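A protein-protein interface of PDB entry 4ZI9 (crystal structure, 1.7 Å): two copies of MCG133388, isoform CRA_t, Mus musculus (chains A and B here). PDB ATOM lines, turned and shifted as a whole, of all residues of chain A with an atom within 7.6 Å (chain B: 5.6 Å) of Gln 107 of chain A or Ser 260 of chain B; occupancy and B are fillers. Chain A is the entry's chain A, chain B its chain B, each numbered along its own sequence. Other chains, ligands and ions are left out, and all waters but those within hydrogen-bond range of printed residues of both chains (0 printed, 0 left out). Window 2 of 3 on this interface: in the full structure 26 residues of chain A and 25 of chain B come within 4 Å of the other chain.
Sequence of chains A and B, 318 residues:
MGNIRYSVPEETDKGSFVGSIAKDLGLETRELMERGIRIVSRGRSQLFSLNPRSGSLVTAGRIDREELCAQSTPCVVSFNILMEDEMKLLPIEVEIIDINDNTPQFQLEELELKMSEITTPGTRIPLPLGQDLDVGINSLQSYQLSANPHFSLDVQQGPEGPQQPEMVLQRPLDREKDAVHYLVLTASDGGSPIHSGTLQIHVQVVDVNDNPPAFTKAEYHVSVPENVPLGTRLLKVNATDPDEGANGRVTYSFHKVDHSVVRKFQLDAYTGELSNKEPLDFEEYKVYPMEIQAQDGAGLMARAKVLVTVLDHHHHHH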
ATOM      1  N   GLN A 105     -18.768   7.421  11.081  1.00  0.00           N
ATOM      2  CA  GLN A 105     -17.789   8.488  11.223  1.00  0.00           C
ATOM      3  C   GLN A 105     -16.373   8.002  10.940  1.00  0.00           C
ATOM      4  O   GLN A 105     -15.994   6.881  11.296  1.00  0.00           O
ATOM      5  CB  GLN A 105     -17.822   9.077  12.636  1.00  0.00           C
ATOM      6  CG  GLN A 105     -19.130   9.749  12.986  1.00  0.00           C
ATOM      7  CD  GLN A 105     -19.441  10.872  12.038  1.00  0.00           C
ATOM      8  OE1 GLN A 105     -18.690  11.845  11.937  1.00  0.00           O
ATOM      9  NE2 GLN A 105     -20.524  10.726  11.298  1.00  0.00           N
ATOM     10  N   PHE A 106     -15.597   8.862  10.298  1.00  0.00           N
ATOM     11  CA  PHE A 106     -14.164   8.665  10.186  1.00  0.00           C
ATOM     12  C   PHE A 106     -13.534   9.512  11.264  1.00  0.00           C
ATOM     13  O   PHE A 106     -14.150  10.460  11.754  1.00  0.00           O
ATOM     14  CB  PHE A 106     -13.646   9.064   8.807  1.00  0.00           C
ATOM     15  CG  PHE A 106     -14.158   8.196   7.697  1.00  0.00           C
ATOM     16  CD1 PHE A 106     -13.538   6.981   7.405  1.00  0.00           C
ATOM     17  CD2 PHE A 106     -15.234   8.594   6.946  1.00  0.00           C
ATOM     18  CE1 PHE A 106     -14.023   6.168   6.383  1.00  0.00           C
ATOM     19  CE2 PHE A 106     -15.734   7.796   5.915  1.00  0.00           C
ATOM     20  CZ  PHE A 106     -15.110   6.572   5.639  1.00  0.00           C
ATOM     21  N   GLN A 107     -12.306   9.179  11.622  1.00  0.00           N
ATOM     22  CA  GLN A 107     -11.614   9.868  12.686  1.00  0.00           C
ATOM     23  C   GLN A 107     -10.765  11.010  12.148  1.00  0.00           C
ATOM     24  O   GLN A 107     -10.006  11.625  12.888  1.00  0.00           O
ATOM     25  CB  GLN A 107     -10.779   8.865  13.479  1.00  0.00           C
ATOM     26  CG  GLN A 107     -11.676   7.891  14.281  1.00  0.00           C
ATOM     27  CD  GLN A 107     -10.914   6.744  14.933  1.00  0.00           C
ATOM     28  OE1 GLN A 107     -10.640   5.723  14.299  1.00  0.00           O
ATOM     29  NE2 GLN A 107     -10.585   6.904  16.212  1.00  0.00           N
ATOM     30  N   LEU A 108     -10.892  11.283  10.852  1.00  0.00           N
ATOM     31  CA  LEU A 108     -10.269  12.451  10.227  1.00  0.00           C
ATOM     32  C   LEU A 108     -11.087  12.863   8.999  1.00  0.00           C
ATOM     33  O   LEU A 108     -11.857  12.067   8.453  1.00  0.00           O
ATOM     34  CB  LEU A 108      -8.810  12.164   9.827  1.00  0.00           C
ATOM     35  CG  LEU A 108      -8.568  11.335   8.565  1.00  0.00           C
ATOM     36  CD1 LEU A 108      -7.095  11.372   8.198  1.00  0.00           C
ATOM     37  CD2 LEU A 108      -9.047   9.900   8.735  1.00  0.00           C
ATOM     38  N   GLU A 109     -10.916  14.096   8.548  1.00  0.00           N
ATOM     39  CA  GLU A 109     -11.678  14.583   7.397  1.00  0.00           C
ATOM     40  C   GLU A 109     -11.013  14.372   6.027  1.00  0.00           C
ATOM     41  O   GLU A 109     -11.694  14.070   5.032  1.00  0.00           O
ATOM     42  CB  GLU A 109     -11.991  16.063   7.596  1.00  0.00           C
ATOM     43  CG  GLU A 109     -12.938  16.295   8.763  1.00  0.00           C
ATOM     44  CD  GLU A 109     -13.341  17.737   8.913  1.00  0.00           C
ATOM     45  OE1 GLU A 109     -12.457  18.618   8.836  1.00  0.00           O
ATOM     46  OE2 GLU A 109     -14.550  17.988   9.093  1.00  0.00           O
ATOM     47  N   GLU A 110      -9.702  14.537   5.959  1.00  0.00           N
ATOM     48  CA  GLU A 110      -9.019  14.375   4.684  1.00  0.00           C
ATOM     49  C   GLU A 110      -7.740  13.567   4.845  1.00  0.00           C
ATOM     50  O   GLU A 110      -6.901  13.862   5.699  1.00  0.00           O
ATOM     51  CB  GLU A 110      -8.718  15.738   4.040  1.00  0.00           C
ATOM     52  CG  GLU A 110      -7.888  15.622   2.721  1.00  0.00           C
ATOM     53  CD  GLU A 110      -8.000  16.839   1.803  1.00  0.00           C
ATOM     54  OE1 GLU A 110      -7.133  16.998   0.913  1.00  0.00           O
ATOM     55  OE2 GLU A 110      -8.965  17.623   1.962  1.00  0.00           O
ATOM     56  N   PRO A 128      -8.656   4.645   6.317  1.00  0.00           N
ATOM     57  CA  PRO A 128      -9.191   4.891   7.653  1.00  0.00           C
ATOM     58  C   PRO A 128     -10.530   4.186   7.826  1.00  0.00           C
ATOM     59  O   PRO A 128     -11.294   4.095   6.867  1.00  0.00           O
ATOM     60  CB  PRO A 128      -9.340   6.415   7.704  1.00  0.00           C
ATOM     61  CG  PRO A 128      -8.352   6.929   6.681  1.00  0.00           C
ATOM     62  CD  PRO A 128      -8.392   5.899   5.583  1.00  0.00           C
ATOM     63  N   LEU A 129     -10.794   3.678   9.023  1.00  0.00           N
ATOM     64  CA  LEU A 129     -12.043   2.958   9.287  1.00  0.00           C
ATOM     65  C   LEU A 129     -13.233   3.886   9.522  1.00  0.00           C
ATOM     66  O   LEU A 129     -13.107   4.944  10.127  1.00  0.00           O
ATOM     67  CB  LEU A 129     -11.887   2.052  10.507  1.00  0.00           C
ATOM     68  CG  LEU A 129     -10.795   0.989  10.518  1.00  0.00           C
ATOM     69  CD1 LEU A 129     -11.054   0.077  11.730  1.00  0.00           C
ATOM     70  CD2 LEU A 129     -10.863   0.212   9.240  1.00  0.00           C
ATOM     71  N   GLY A 130     -14.393   3.482   9.050  1.00  0.00           N
ATOM     72  CA  GLY A 130     -15.619   4.156   9.456  1.00  0.00           C
ATOM     73  C   GLY A 130     -16.198   3.416  10.649  1.00  0.00           C
ATOM     74  O   GLY A 130     -16.144   2.188  10.705  1.00  0.00           O
ATOM     75  N   GLN A 131     -16.777   4.158  11.590  1.00  0.00           N
ATOM     76  CA  GLN A 131     -17.358   3.585  12.801  1.00  0.00           C
ATOM     77  C   GLN A 131     -18.744   4.196  13.051  1.00  0.00           C
ATOM     78  O   GLN A 131     -18.891   5.417  13.130  1.00  0.00           O
ATOM     79  CB  GLN A 131     -16.438   3.833  13.989  1.00  0.00           C
ATOM     80  CG  GLN A 131     -17.074   3.618  15.358  1.00  0.00           C
ATOM     81  CD  GLN A 131     -16.167   4.085  16.491  1.00  0.00           C
ATOM     82  OE1 GLN A 131     -16.633   4.648  17.489  1.00  0.00           O
ATOM     83  NE2 GLN A 131     -14.857   3.862  16.332  1.00  0.00           N
ATOM     84  N   LEU A 199     -15.081  10.623   3.636  1.00  0.00           N
ATOM     85  CA  LEU A 199     -13.674  10.938   3.804  1.00  0.00           C
ATOM     86  C   LEU A 199     -13.111  11.460   2.462  1.00  0.00           C
ATOM     87  O   LEU A 199     -13.301  10.831   1.405  1.00  0.00           O
ATOM     88  CB  LEU A 199     -12.910   9.709   4.285  1.00  0.00           C
ATOM     89  CG  LEU A 199     -11.388   9.834   4.270  1.00  0.00           C
ATOM     90  CD1 LEU A 199     -10.904  10.742   5.387  1.00  0.00           C
ATOM     91  CD2 LEU A 199     -10.733   8.463   4.358  1.00  0.00           C
ATOM     92  N   VAL B 257      -5.604   4.110  10.110  1.00  0.00           N
ATOM     93  CA  VAL B 257      -6.597   3.066   9.959  1.00  0.00           C
ATOM     94  C   VAL B 257      -7.561   3.197  11.123  1.00  0.00           C
ATOM     95  O   VAL B 257      -8.620   3.818  11.001  1.00  0.00           O
ATOM     96  CB  VAL B 257      -5.959   1.660   9.939  1.00  0.00           C
ATOM     97  CG1 VAL B 257      -7.030   0.577   9.872  1.00  0.00           C
ATOM     98  CG2 VAL B 257      -4.989   1.534   8.756  1.00  0.00           C
ATOM     99  N   ASP B 258      -7.155   2.693  12.282  1.00  0.00           N
ATOM    100  CA  ASP B 258      -7.964   2.862  13.487  1.00  0.00           C
ATOM    101  C   ASP B 258      -7.196   3.689  14.493  1.00  0.00           C
ATOM    102  O   ASP B 258      -6.368   3.157  15.227  1.00  0.00           O
ATOM    103  CB  ASP B 258      -8.323   1.510  14.085  1.00  0.00           C
ATOM    104  CG  ASP B 258      -9.243   1.628  15.295  1.00  0.00           C
ATOM    105  OD1 ASP B 258      -9.530   2.774  15.735  1.00  0.00           O
ATOM    106  OD2 ASP B 258      -9.661   0.564  15.804  1.00  0.00           O
ATOM    107  N   HIS B 259      -7.482   4.984  14.554  1.00  0.00           N
ATOM    108  CA  HIS B 259      -6.690   5.860  15.403  1.00  0.00           C
ATOM    109  C   HIS B 259      -6.874   5.551  16.894  1.00  0.00           C
ATOM    110  O   HIS B 259      -6.022   5.893  17.716  1.00  0.00           O
ATOM    111  CB  HIS B 259      -7.022   7.317  15.126  1.00  0.00           C
ATOM    112  CG  HIS B 259      -6.106   8.275  15.817  1.00  0.00           C
ATOM    113  ND1 HIS B 259      -4.792   8.446  15.441  1.00  0.00           N
ATOM    114  CD2 HIS B 259      -6.309   9.109  16.863  1.00  0.00           C
ATOM    115  CE1 HIS B 259      -4.225   9.343  16.225  1.00  0.00           C
ATOM    116  NE2 HIS B 259      -5.125   9.763  17.096  1.00  0.00           N
ATOM    117  N   SER B 260      -7.975   4.899  17.249  1.00  0.00           N
ATOM    118  CA  SER B 260      -8.217   4.620  18.660  1.00  0.00           C
ATOM    119  C   SER B 260      -7.182   3.626  19.183  1.00  0.00           C
ATOM    120  O   SER B 260      -6.892   3.591  20.378  1.00  0.00           O
ATOM    121  CB  SER B 260      -9.635   4.083  18.885  1.00  0.00           C
ATOM    122  OG  SER B 260      -9.740   2.712  18.523  1.00  0.00           O
ATOM    123  N   VAL B 261      -6.624   2.820  18.285  1.00  0.00           N
ATOM    124  CA  VAL B 261      -5.563   1.894  18.664  1.00  0.00           C
ATOM    125  C   VAL B 261      -4.200   2.570  18.618  1.00  0.00           C
ATOM    126  O   VAL B 261      -3.456   2.582  19.602  1.00  0.00           O
ATOM    127  CB  VAL B 261      -5.549   0.655  17.753  1.00  0.00           C
ATOM    128  CG1 VAL B 261      -4.311  -0.190  18.025  1.00  0.00           C
ATOM    129  CG2 VAL B 261      -6.813  -0.157  17.963  1.00  0.00           C
ATOM    130  N   VAL B 262      -3.899   3.160  17.468  1.00  0.00           N
ATOM    131  CA  VAL B 262      -2.598   3.749  17.193  1.00  0.00           C
ATOM    132  C   VAL B 262      -2.255   4.900  18.147  1.00  0.00           C
ATOM    133  O   VAL B 262      -1.082   5.119  18.467  1.00  0.00           O
ATOM    134  CB  VAL B 262      -2.556   4.203  15.702  1.00  0.00           C
ATOM    135  CG1 VAL B 262      -1.610   5.353  15.477  1.00  0.00           C
ATOM    136  CG2 VAL B 262      -2.236   3.006  14.823  1.00  0.00           C
ATOM    137  N   ARG B 263      -3.269   5.590  18.668  1.00  0.00           N
ATOM    138  CA  ARG B 263      -3.016   6.715  19.574  1.00  0.00           C
ATOM    139  C   ARG B 263      -2.325   6.292  20.867  1.00  0.00           C
ATOM    140  O   ARG B 263      -1.727   7.124  21.550  1.00  0.00           O
ATOM    141  CB  ARG B 263      -4.323   7.426  19.926  1.00  0.00           C
ATOM    142  CG  ARG B 263      -5.242   6.603  20.798  1.00  0.00           C
ATOM    143  CD  ARG B 263      -6.554   7.326  21.116  1.00  0.00           C
ATOM    144  NE  ARG B 263      -6.552   8.016  22.408  1.00  0.00           N
ATOM    145  CZ  ARG B 263      -6.551   9.339  22.570  1.00  0.00           C
ATOM    146  NH1 ARG B 263      -6.561  10.148  21.518  1.00  0.00           N
ATOM    147  NH2 ARG B 263      -6.554   9.853  23.796  1.00  0.00           N
ATOM    148  N   LYS B 264      -2.405   5.009  21.208  1.00  0.00           N
ATOM    149  CA  LYS B 264      -1.756   4.496  22.421  1.00  0.00           C
ATOM    150  C   LYS B 264      -0.239   4.292  22.230  1.00  0.00           C
ATOM    151  O   LYS B 264       0.478   3.947  23.177  1.00  0.00           O
ATOM    152  CB  LYS B 264      -2.418   3.189  22.842  1.00  0.00           C
ATOM    153  CG  LYS B 264      -3.927   3.379  23.086  1.00  0.00           C
ATOM    154  CD  LYS B 264      -4.589   2.170  23.697  1.00  0.00           C
ATOM    155  CE  LYS B 264      -6.054   2.470  23.995  1.00  0.00           C
ATOM    156  NZ  LYS B 264      -6.716   1.374  24.776  1.00  0.00           N
ATOM    157  N   TYR B 285      -8.820  -4.217  24.977  1.00  0.00           N
ATOM    158  CA  TYR B 285      -8.068  -4.719  23.840  1.00  0.00           C
ATOM    159  C   TYR B 285      -7.084  -5.801  24.286  1.00  0.00           C
ATOM    160  O   TYR B 285      -6.030  -5.490  24.840  1.00  0.00           O
ATOM    161  CB  TYR B 285      -7.291  -3.596  23.165  1.00  0.00           C
ATOM    162  CG  TYR B 285      -8.064  -2.663  22.266  1.00  0.00           C
ATOM    163  CD1 TYR B 285      -8.239  -2.948  20.919  1.00  0.00           C
ATOM    164  CD2 TYR B 285      -8.565  -1.459  22.755  1.00  0.00           C
ATOM    165  CE1 TYR B 285      -8.927  -2.076  20.088  1.00  0.00           C
ATOM    166  CE2 TYR B 285      -9.251  -0.580  21.932  1.00  0.00           C
ATOM    167  CZ  TYR B 285      -9.430  -0.894  20.599  1.00  0.00           C
ATOM    168  OH  TYR B 285     -10.113  -0.027  19.774  1.00  0.00           O
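Among the printed residues, no Asp or Glu carboxylate lies within 4 Å of a Lys or Arg side-chain nitrogen of the other chain.
No position is printed for both chains. Of the 6 pairs that touch across the chains among the printed residues, none has its exchanged pair printed and touching as well.
The side-chain hydroxyl of Ser 260 of chain B is in hydrogen-bond range of the side-chain carboxylate of Asp 258 of chain B, 2.8 Å away. The side-chain hydroxyl (OG) of Ser 260 of chain B is in hydrogen-bond range of the side-chain hydroxyl (OH) of Tyr 285 of chain B.
Among the printed residues, merely in contact across the chains: Pro 128 of chain A with Val 257 of chain B (3.6 Å) and Leu 129 of chain A with Asp 258 of chain B (3.9 Å).
Of the printed residues of chain B, Gln 107 of chain A touches Asp 258 (3.5 Å), His 259 (3.3 Å) and Ser 260 (3.5 Å). Printed residues of chain A within 4 Å of Ser 260 of chain B: Gln 107 (3.5 Å). Printed residues of chain B within 4 Å of Pro 128 of chain A: Val 257. Of the printed residues of chain A, His 259 of chain B touches Gln 107 (3.3 Å). Of the printed residues of chain B, Leu 129 of chain A touches Val 257 (2.9 Å) and Asp 258 (3.9 Å). Of the printed residues of chain A, Val 257 of chain B touches Pro 128 and Leu 129. The nearest residue of chain B that does not touch Gln 107 of chain A is Val 257 of chain B (4.3 Å). The nearest residue of chain A that does not touch Ser 260 of chain B is Gln 131 of chain A (5.7 Å). The nearest printed residue of chain B that does not touch Leu 129 of chain A is His 259 of chain B (6.6 Å).
The side-chain amide oxygen (OE1) of Gln 107 of chain A lies close to the side-chain carboxylate (OD1) of Asp 258 of chain B. NE2 of Gln 107 of chain A lies close to N of Ser 260 of chain B, at 3.5 Å. The side-chain amide oxygen (OE1) of Gln 107 of chain A lies within hydrogen-bond range of the backbone NH (N) of His 259 of chain B, 3.3 Å away. The backbone NH (N) of Leu 129 of chain A sits at hydrogen-bond distance from the backbone carbonyl oxygen (O) of Val 257 of chain B (2.9 Å).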
